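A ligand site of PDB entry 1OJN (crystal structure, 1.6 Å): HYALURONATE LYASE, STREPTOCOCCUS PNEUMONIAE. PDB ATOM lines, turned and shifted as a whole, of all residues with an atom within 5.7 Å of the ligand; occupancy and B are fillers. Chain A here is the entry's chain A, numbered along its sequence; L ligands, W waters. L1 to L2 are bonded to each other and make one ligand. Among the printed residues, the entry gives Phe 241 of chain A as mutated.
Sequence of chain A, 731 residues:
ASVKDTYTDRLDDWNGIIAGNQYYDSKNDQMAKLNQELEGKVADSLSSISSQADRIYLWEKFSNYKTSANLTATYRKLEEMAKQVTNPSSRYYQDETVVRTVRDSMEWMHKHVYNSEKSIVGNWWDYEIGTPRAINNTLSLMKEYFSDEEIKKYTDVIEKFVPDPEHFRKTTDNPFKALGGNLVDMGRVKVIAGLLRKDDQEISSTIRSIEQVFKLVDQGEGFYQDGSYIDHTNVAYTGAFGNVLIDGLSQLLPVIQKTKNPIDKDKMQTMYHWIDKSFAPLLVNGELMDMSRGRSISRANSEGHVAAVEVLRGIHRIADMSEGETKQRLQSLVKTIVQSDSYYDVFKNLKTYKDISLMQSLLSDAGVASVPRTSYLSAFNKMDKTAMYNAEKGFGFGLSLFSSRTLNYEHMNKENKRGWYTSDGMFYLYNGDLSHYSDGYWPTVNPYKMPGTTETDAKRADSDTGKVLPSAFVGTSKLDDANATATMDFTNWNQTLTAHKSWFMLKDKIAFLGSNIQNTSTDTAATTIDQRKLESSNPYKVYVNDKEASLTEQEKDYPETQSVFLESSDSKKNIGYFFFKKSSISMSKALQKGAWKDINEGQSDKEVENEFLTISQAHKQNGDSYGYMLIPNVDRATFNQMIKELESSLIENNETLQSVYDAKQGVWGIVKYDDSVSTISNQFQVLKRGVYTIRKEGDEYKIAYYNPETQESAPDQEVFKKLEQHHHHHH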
ATOM      1  N   ALA A  69      17.171  10.649  -1.122  1.00  0.00           N
ATOM      2  CA  ALA A  69      15.761  10.913  -1.433  1.00  0.00           C
ATOM      3  C   ALA A  69      15.561  12.278  -2.096  1.00  0.00           C
ATOM      4  O   ALA A  69      14.634  12.467  -2.886  1.00  0.00           O
ATOM      5  CB  ALA A  69      14.926  10.840  -0.157  1.00  0.00           C
ATOM      6  N   ARG A  76      11.995  14.355 -10.114  1.00  0.00           N
ATOM      7  CA  ARG A  76      10.577  14.108 -10.384  1.00  0.00           C
ATOM      8  C   ARG A  76       9.839  15.420 -10.620  1.00  0.00           C
ATOM      9  O   ARG A  76       8.828  15.447 -11.329  1.00  0.00           O
ATOM     10  CB  ARG A  76       9.948  13.319  -9.238  1.00  0.00           C
ATOM     11  CG  ARG A  76      10.327  11.849  -9.281  1.00  0.00           C
ATOM     12  CD  ARG A  76       9.612  11.027  -8.219  1.00  0.00           C
ATOM     13  NE  ARG A  76       9.890   9.607  -8.417  1.00  0.00           N
ATOM     14  CZ  ARG A  76       9.470   8.640  -7.614  1.00  0.00           C
ATOM     15  NH1 ARG A  76       9.772   7.373  -7.883  1.00  0.00           N
ATOM     16  NH2 ARG A  76       8.746   8.929  -6.543  1.00  0.00           N
ATOM     17  N   ASN A 123      20.741   6.013  -0.014  1.00  0.00           N
ATOM     18  CA  ASN A 123      19.999   4.859  -0.512  1.00  0.00           C
ATOM     19  C   ASN A 123      20.340   4.562  -1.985  1.00  0.00           C
ATOM     20  O   ASN A 123      20.167   5.418  -2.846  1.00  0.00           O
ATOM     21  CB  ASN A 123      18.492   5.122  -0.388  1.00  0.00           C
ATOM     22  CG  ASN A 123      17.667   3.852  -0.454  1.00  0.00           C
ATOM     23  OD1 ASN A 123      18.039   2.882  -1.126  1.00  0.00           O
ATOM     24  ND2 ASN A 123      16.524   3.852   0.227  1.00  0.00           N
ATOM     25  N   TRP A 125      18.760   2.807  -4.001  1.00  0.00           N
ATOM     26  CA  TRP A 125      17.543   2.830  -4.796  1.00  0.00           C
ATOM     27  C   TRP A 125      17.344   4.130  -5.563  1.00  0.00           C
ATOM     28  O   TRP A 125      16.882   4.126  -6.704  1.00  0.00           O
ATOM     29  CB  TRP A 125      16.334   2.585  -3.896  1.00  0.00           C
ATOM     30  CG  TRP A 125      15.061   2.383  -4.659  1.00  0.00           C
ATOM     31  CD1 TRP A 125      14.544   1.195  -5.085  1.00  0.00           C
ATOM     32  CD2 TRP A 125      14.147   3.397  -5.090  1.00  0.00           C
ATOM     33  NE1 TRP A 125      13.362   1.411  -5.762  1.00  0.00           N
ATOM     34  CE2 TRP A 125      13.099   2.754  -5.776  1.00  0.00           C
ATOM     35  CE3 TRP A 125      14.113   4.800  -4.962  1.00  0.00           C
ATOM     36  CZ2 TRP A 125      12.018   3.451  -6.338  1.00  0.00           C
ATOM     37  CZ3 TRP A 125      13.042   5.496  -5.521  1.00  0.00           C
ATOM     38  CH2 TRP A 125      12.017   4.816  -6.196  1.00  0.00           C
ATOM     39  N   ASP A 126      17.686   5.249  -4.923  1.00  0.00           N
ATOM     40  CA  ASP A 126      17.542   6.551  -5.560  1.00  0.00           C
ATOM     41  C   ASP A 126      18.539   6.720  -6.699  1.00  0.00           C
ATOM     42  O   ASP A 126      18.220   7.303  -7.736  1.00  0.00           O
ATOM     43  CB  ASP A 126      17.751   7.677  -4.540  1.00  0.00           C
ATOM     44  CG  ASP A 126      16.618   7.775  -3.546  1.00  0.00           C
ATOM     45  OD1 ASP A 126      15.464   8.012  -3.968  1.00  0.00           O
ATOM     46  OD2 ASP A 126      16.871   7.624  -2.323  1.00  0.00           O
ATOM     47  N   ARG A 133      14.797   6.666 -13.456  1.00  0.00           N
ATOM     48  CA  ARG A 133      13.474   6.610 -14.058  1.00  0.00           C
ATOM     49  C   ARG A 133      12.964   8.021 -14.329  1.00  0.00           C
ATOM     50  O   ARG A 133      12.377   8.282 -15.382  1.00  0.00           O
ATOM     51  CB  ARG A 133      12.493   5.879 -13.146  1.00  0.00           C
ATOM     52  CG  ARG A 133      12.567   4.356 -13.225  1.00  0.00           C
ATOM     53  CD  ARG A 133      11.777   3.718 -12.099  1.00  0.00           C
ATOM     54  NE  ARG A 133      10.443   4.298 -11.995  1.00  0.00           N
ATOM     55  CZ  ARG A 133       9.689   4.220 -10.909  1.00  0.00           C
ATOM     56  NH1 ARG A 133      10.124   3.578  -9.833  1.00  0.00           N
ATOM     57  NH2 ARG A 133       8.487   4.794 -10.890  1.00  0.00           N
ATOM     58  N   ARG A 188      12.398  -0.419 -16.609  1.00  0.00           N
ATOM     59  CA  ARG A 188      12.014   0.979 -16.751  1.00  0.00           C
ATOM     60  C   ARG A 188      13.225   1.894 -16.702  1.00  0.00           C
ATOM     61  O   ARG A 188      13.135   3.085 -17.031  1.00  0.00           O
ATOM     62  CB  ARG A 188      11.003   1.365 -15.661  1.00  0.00           C
ATOM     63  CG  ARG A 188       9.667   0.626 -15.830  1.00  0.00           C
ATOM     64  CD  ARG A 188       8.539   1.272 -15.044  1.00  0.00           C
ATOM     65  NE  ARG A 188       8.668   1.120 -13.603  1.00  0.00           N
ATOM     66  CZ  ARG A 188       7.748   1.519 -12.729  1.00  0.00           C
ATOM     67  NH1 ARG A 188       6.642   2.109 -13.163  1.00  0.00           N
ATOM     68  NH2 ARG A 188       7.940   1.348 -11.424  1.00  0.00           N
ATOM     69  N   HIS A 232      12.606  -9.739  -0.701  1.00  0.00           N
ATOM     70  CA  HIS A 232      13.525  -9.483   0.397  1.00  0.00           C
ATOM     71  C   HIS A 232      13.838 -10.763   1.177  1.00  0.00           C
ATOM     72  O   HIS A 232      13.701 -10.817   2.404  1.00  0.00           O
ATOM     73  CB  HIS A 232      12.957  -8.416   1.329  1.00  0.00           C
ATOM     74  CG  HIS A 232      13.018  -7.032   0.754  1.00  0.00           C
ATOM     75  ND1 HIS A 232      12.551  -5.920   1.428  1.00  0.00           N
ATOM     76  CD2 HIS A 232      13.527  -6.582  -0.412  1.00  0.00           C
ATOM     77  CE1 HIS A 232      12.766  -4.842   0.688  1.00  0.00           C
ATOM     78  NE2 HIS A 232      13.354  -5.213  -0.430  1.00  0.00           N
ATOM     79  N   TYR A 237       5.162 -10.437   0.247  1.00  0.00           N
ATOM     80  CA  TYR A 237       5.161  -9.083  -0.314  1.00  0.00           C
ATOM     81  C   TYR A 237       4.371  -8.809  -1.590  1.00  0.00           C
ATOM     82  O   TYR A 237       4.668  -7.847  -2.308  1.00  0.00           O
ATOM     83  CB  TYR A 237       6.621  -8.656  -0.552  1.00  0.00           C
ATOM     84  CG  TYR A 237       7.070  -7.489   0.303  1.00  0.00           C
ATOM     85  CD1 TYR A 237       6.257  -6.360   0.441  1.00  0.00           C
ATOM     86  CD2 TYR A 237       8.307  -7.501   0.944  1.00  0.00           C
ATOM     87  CE1 TYR A 237       6.656  -5.281   1.212  1.00  0.00           C
ATOM     88  CE2 TYR A 237       8.725  -6.415   1.724  1.00  0.00           C
ATOM     89  CZ  TYR A 237       7.886  -5.299   1.838  1.00  0.00           C
ATOM     90  OH  TYR A 237       8.260  -4.213   2.590  1.00  0.00           O
ATOM     91  N   ALA A 240       3.104  -5.023  -2.248  1.00  0.00           N
ATOM     92  CA  ALA A 240       3.967  -3.845  -2.312  1.00  0.00           C
ATOM     93  C   ALA A 240       4.953  -4.046  -3.462  1.00  0.00           C
ATOM     94  O   ALA A 240       4.875  -3.362  -4.474  1.00  0.00           O
ATOM     95  CB  ALA A 240       4.693  -3.636  -1.001  1.00  0.00           C
ATOM     96  N   PHE A 241       5.860  -5.001  -3.313  1.00  0.00           N
ATOM     97  CA  PHE A 241       6.804  -5.260  -4.395  1.00  0.00           C
ATOM     98  C   PHE A 241       6.100  -5.961  -5.551  1.00  0.00           C
ATOM     99  O   PHE A 241       6.485  -5.799  -6.704  1.00  0.00           O
ATOM    100  CB  PHE A 241       8.008  -6.060  -3.903  1.00  0.00           C
ATOM    101  CG  PHE A 241       9.028  -5.222  -3.199  1.00  0.00           C
ATOM    102  CD1 PHE A 241       8.973  -5.044  -1.817  1.00  0.00           C
ATOM    103  CD2 PHE A 241      10.002  -4.544  -3.920  1.00  0.00           C
ATOM    104  CE1 PHE A 241       9.872  -4.203  -1.167  1.00  0.00           C
ATOM    105  CE2 PHE A 241      10.909  -3.699  -3.288  1.00  0.00           C
ATOM    106  CZ  PHE A 241      10.844  -3.528  -1.912  1.00  0.00           C
ATOM    107  N   VAL A 244       4.562  -3.153  -7.596  1.00  0.00           N
ATOM    108  CA  VAL A 244       5.547  -2.516  -8.466  1.00  0.00           C
ATOM    109  C   VAL A 244       5.776  -3.373  -9.697  1.00  0.00           C
ATOM    110  O   VAL A 244       5.873  -2.869 -10.812  1.00  0.00           O
ATOM    111  CB  VAL A 244       6.886  -2.317  -7.712  1.00  0.00           C
ATOM    112  CG1 VAL A 244       7.946  -1.776  -8.667  1.00  0.00           C
ATOM    113  CG2 VAL A 244       6.682  -1.361  -6.546  1.00  0.00           C
ATOM    114  N   ARG A 295       6.173  -3.246   4.796  1.00  0.00           N
ATOM    115  CA  ARG A 295       6.358  -1.961   5.476  1.00  0.00           C
ATOM    116  C   ARG A 295       5.571  -0.797   4.889  1.00  0.00           C
ATOM    117  O   ARG A 295       5.503   0.278   5.490  1.00  0.00           O
ATOM    118  CB  ARG A 295       7.848  -1.608   5.537  1.00  0.00           C
ATOM    119  CG  ARG A 295       8.480  -1.165   4.216  1.00  0.00           C
ATOM    120  CD  ARG A 295       9.967  -0.865   4.426  1.00  0.00           C
ATOM    121  NE  ARG A 295      10.524  -0.032   3.364  1.00  0.00           N
ATOM    122  CZ  ARG A 295      11.132  -0.485   2.275  1.00  0.00           C
ATOM    123  NH1 ARG A 295      11.286  -1.794   2.083  1.00  0.00           N
ATOM    124  NH2 ARG A 295      11.597   0.362   1.370  1.00  0.00           N
ATOM    125  N   SER A 296       4.959  -1.001   3.719  1.00  0.00           N
ATOM    126  CA  SER A 296       4.184   0.053   3.074  1.00  0.00           C
ATOM    127  C   SER A 296       2.931   0.447   3.860  1.00  0.00           C
ATOM    128  O   SER A 296       2.343   1.489   3.586  1.00  0.00           O
ATOM    129  CB  SER A 296       3.772  -0.378   1.667  1.00  0.00           C
ATOM    130  OG  SER A 296       4.908  -0.434   0.816  1.00  0.00           O
ATOM    131  N   ARG A 299       2.805   4.020   5.397  1.00  0.00           N
ATOM    132  CA  ARG A 299       2.808   5.207   4.543  1.00  0.00           C
ATOM    133  C   ARG A 299       1.390   5.759   4.467  1.00  0.00           C
ATOM    134  O   ARG A 299       0.476   5.084   4.008  1.00  0.00           O
ATOM    135  CB  ARG A 299       3.317   4.846   3.147  1.00  0.00           C
ATOM    136  CG  ARG A 299       4.739   4.348   3.140  1.00  0.00           C
ATOM    137  CD  ARG A 299       5.139   3.821   1.771  1.00  0.00           C
ATOM    138  NE  ARG A 299       6.464   3.202   1.807  1.00  0.00           N
ATOM    139  CZ  ARG A 299       6.954   2.442   0.838  1.00  0.00           C
ATOM    140  NH1 ARG A 299       6.231   2.189  -0.243  1.00  0.00           N
ATOM    141  NH2 ARG A 299       8.162   1.914   0.953  1.00  0.00           N
ATOM    142  N   SER A 302      -0.526   5.694   1.177  1.00  0.00           N
ATOM    143  CA  SER A 302      -0.665   4.375   0.571  1.00  0.00           C
ATOM    144  C   SER A 302      -1.517   3.399   1.358  1.00  0.00           C
ATOM    145  O   SER A 302      -1.145   2.246   1.525  1.00  0.00           O
ATOM    146  CB  SER A 302       0.720   3.761   0.356  1.00  0.00           C
ATOM    147  OG  SER A 302       1.522   4.560  -0.495  1.00  0.00           O
ATOM    148  N   GLU A 310      -2.891   0.479  -7.652  1.00  0.00           N
ATOM    149  CA  GLU A 310      -1.657   0.181  -8.365  1.00  0.00           C
ATOM    150  C   GLU A 310      -1.832  -1.161  -9.068  1.00  0.00           C
ATOM    151  O   GLU A 310      -1.413  -1.350 -10.201  1.00  0.00           O
ATOM    152  CB  GLU A 310      -0.465   0.053  -7.410  1.00  0.00           C
ATOM    153  CG  GLU A 310      -0.029   1.312  -6.733  1.00  0.00           C
ATOM    154  CD  GLU A 310       1.327   1.142  -6.079  1.00  0.00           C
ATOM    155  OE1 GLU A 310       1.475   0.192  -5.284  1.00  0.00           O
ATOM    156  OE2 GLU A 310       2.232   1.950  -6.354  1.00  0.00           O
ATOM    157  N   ASN A 413      14.588   1.148   6.360  1.00  0.00           N
ATOM    158  CA  ASN A 413      14.536   2.499   5.823  1.00  0.00           C
ATOM    159  C   ASN A 413      13.653   3.352   6.739  1.00  0.00           C
ATOM    160  O   ASN A 413      12.975   4.281   6.295  1.00  0.00           O
ATOM    161  CB  ASN A 413      13.998   2.508   4.395  1.00  0.00           C
ATOM    162  CG  ASN A 413      14.917   1.773   3.423  1.00  0.00           C
ATOM    163  OD1 ASN A 413      16.139   1.842   3.554  1.00  0.00           O
ATOM    164  ND2 ASN A 413      14.338   1.086   2.447  1.00  0.00           N
ATOM    165  N   GLU A 415      10.948   2.607   8.218  1.00  0.00           N
ATOM    166  CA  GLU A 415       9.522   2.418   8.004  1.00  0.00           C
ATOM    167  C   GLU A 415       8.997   1.203   8.750  1.00  0.00           C
ATOM    168  O   GLU A 415       9.681   0.188   8.869  1.00  0.00           O
ATOM    169  CB  GLU A 415       9.235   2.245   6.500  1.00  0.00           C
ATOM    170  CG  GLU A 415       9.662   3.424   5.644  1.00  0.00           C
ATOM    171  CD  GLU A 415       9.139   3.328   4.217  1.00  0.00           C
ATOM    172  OE1 GLU A 415       9.646   2.479   3.449  1.00  0.00           O
ATOM    173  OE2 GLU A 415       8.213   4.090   3.869  1.00  0.00           O
HETATM  174  C1  LIG L   1      11.701   1.003  -2.278  1.00  0.00           C
HETATM  175  C2  LIG L   1      10.167   1.179  -2.175  1.00  0.00           C
HETATM  176  C3  LIG L   1       9.772   2.477  -2.926  1.00  0.00           C
HETATM  177  C4  LIG L   1      10.515   3.735  -2.280  1.00  0.00           C
HETATM  178  C5  LIG L   1      12.034   3.519  -2.388  1.00  0.00           C
HETATM  179  C6  LIG L   1      12.804   4.689  -1.767  1.00  0.00           C
HETATM  180  C7  LIG L   1       8.405  -0.698  -2.002  1.00  0.00           C
HETATM  181  C8  LIG L   1       7.731  -1.814  -2.761  1.00  0.00           C
HETATM  182  N1  LIG L   1       9.406  -0.011  -2.799  1.00  0.00           N
HETATM  183  O1  LIG L   1      12.095  -0.172  -1.595  1.00  0.00           O
HETATM  184  O2  LIG L   1       8.334   2.587  -2.827  1.00  0.00           O
HETATM  185  O3  LIG L   1      10.011   3.835  -0.993  1.00  0.00           O
HETATM  186  O4  LIG L   1      12.412   2.206  -1.691  1.00  0.00           O
HETATM  187  O5  LIG L   1      12.314   5.342  -0.453  1.00  0.00           O
HETATM  188  O6  LIG L   1       8.114  -0.388  -0.813  1.00  0.00           O
HETATM  189  S1  LIG L   1      11.819   6.576   0.199  1.00  0.00           S
HETATM  190  O7  LIG L   1      10.587   6.987  -0.458  1.00  0.00           O
HETATM  191  O8  LIG L   1      12.843   7.645   0.077  1.00  0.00           O
HETATM  192  O9  LIG L   1      11.548   6.305   1.639  1.00  0.00           O
HETATM  193  C1  LG2 L   2       7.552   2.482  -3.978  1.00  0.00           C
HETATM  194  C2  LG2 L   2       6.103   2.608  -3.638  1.00  0.00           C
HETATM  195  C3  LG2 L   2       5.303   2.493  -5.007  1.00  0.00           C
HETATM  196  C4  LG2 L   2       5.841   3.197  -6.272  1.00  0.00           C
HETATM  197  C5  LG2 L   2       7.059   3.831  -6.184  1.00  0.00           C
HETATM  198  C6  LG2 L   2       7.733   4.574  -7.325  1.00  0.00           C
HETATM  199  O1  LG2 L   2       5.728   1.461  -2.799  1.00  0.00           O
HETATM  200  O2  LG2 L   2       3.938   2.723  -4.577  1.00  0.00           O
HETATM  201  O3  LG2 L   2       7.827   3.757  -4.843  1.00  0.00           O
HETATM  202  O4  LG2 L   2       7.127   4.611  -8.464  1.00  0.00           O
HETATM  203  O5  LG2 L   2       8.842   5.094  -6.955  1.00  0.00           O
HETATM  204  O   HOH W   1      15.679   7.006   0.128  1.00  0.00           O
HETATM  205  O   HOH W   2       8.459   5.977   1.904  1.00  0.00           O
HETATM  206  O   HOH W   3       4.008  -0.606  -4.038  1.00  0.00           O
HETATM  207  O   HOH W   4      13.982  -1.989   0.207  1.00  0.00           O
HETATM  208  O   HOH W   5       3.651   2.929  -1.270  1.00  0.00           O
HETATM  209  O   HOH W   6      12.982   8.402  -2.730  1.00  0.00           O
HETATM  210  O   HOH W   7       9.986  -0.154  -5.469  1.00  0.00           O
HETATM  211  O   HOH W   8       7.048  -1.870   1.090  1.00  0.00           O
HETATM  212  O   HOH W   9       3.844   0.044  -1.491  1.00  0.00           O
HETATM  213  O   HOH W  10      14.794  -0.702  -1.827  1.00  0.00           O
HETATM  214  O   HOH W  11      11.478   3.321   1.495  1.00  0.00           O
HETATM  215  O   HOH W  12       4.701   5.089  -9.339  1.00  0.00           O
HETATM  216  O   HOH W  13       9.094   6.490  -4.384  1.00  0.00           O
HETATM  217  O   HOH W  14       7.608   5.419  -1.138  1.00  0.00           O
HETATM  218  O   HOH W  15       6.616   1.822  -9.123  1.00  0.00           O
HETATM  219  O   HOH W  16      14.921   1.772  -0.623  1.00  0.00           O
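The guanidinium group (NH2) of Arg 295 sits close to the side-chain amide nitrogen (ND2) of Asn 413 (3.0 Å).
NE of Arg 295 lies within salt-bridge range of OE1 of Glu 415, 2.7 Å away.
N of Arg 295 sits at hydrogen-bond distance from OH of Tyr 237 (3.2 Å).
The guanidinium group (NE) of Arg 299 is in salt-bridge range of the side-chain carboxylate (OE2) of Glu 415 (2.8 Å).
N of Trp 125 sits at hydrogen-bond distance from OD1 of Asn 123, at 3.0 Å.
N of Ala 69 sits at hydrogen-bond distance from OD2 of Asp 126 (3.3 Å).
The guanidinium group of Arg 299 is in hydrogen-bond range of the side-chain hydroxyl of Ser 296.
Merely in contact with the ligand: Trp 125 (3.3 Å), Phe 241 (3.6 Å), Ser 296 (3.6 Å), Ala 240 (3.6 Å), Ala 69 (3.8 Å) and Val 244 (3.95 Å).
NH2 of Arg 133 is in salt-bridge range of O4 of LG2 L2, 2.8 Å away.
An oxygen (O1) of LIG L1 lies within hydrogen-bond range of the guanidinium group of Arg 295, 3.1 Å away.
The side-chain carboxylate of Glu 310 is in hydrogen-bond range of an oxygen (O2) of LG2 L2 (2.6 Å).
NH1 of Arg 76 is in salt-bridge range of O5 of LG2 L2 (2.6 Å).
The guanidinium group (NH1) of Arg 299 lies within hydrogen-bond range of an oxygen (O1) of LG2 L2 (2.7 Å).
Water W8 lies within hydrogen-bond range of the side-chain hydroxyl (OG) of Ser 296, an oxygen (O6) of LIG L1 and the side-chain hydroxyl (OH) of Tyr 237.
Water W16 lies within hydrogen-bond range of the side-chain amide nitrogen of Asn 123 (2.8 Å), an oxygen (O4) of LIG L1 (2.8 Å) and the side-chain amide nitrogen of Asn 413 (3.2 Å).
Water W1 lies within hydrogen-bond range of the side-chain carboxylate of Asp 126 (2.8 Å), an oxygen (O8) of LIG L1 (2.9 Å) and the side-chain amide nitrogen of Asn 123 (3.3 Å).
Water W11 lies within hydrogen-bond range of OE1 of Glu 415 (2.8 Å), O5 of LIG L1 (2.9 Å) and NH2 of Arg 295 (3.0 Å).
Water W5 lies within hydrogen-bond range of the side-chain hydroxyl (OG) of Ser 302 (2.8 Å), the guanidinium group (NH1) of Arg 299 (2.9 Å) and an oxygen (O1) of LG2 L2 (3.0 Å).
Water W2 lies within hydrogen-bond range of OE2 of Glu 415 (2.7 Å), O9 of LIG L1 (3.1 Å) and NE of Arg 299 (3.4 Å).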
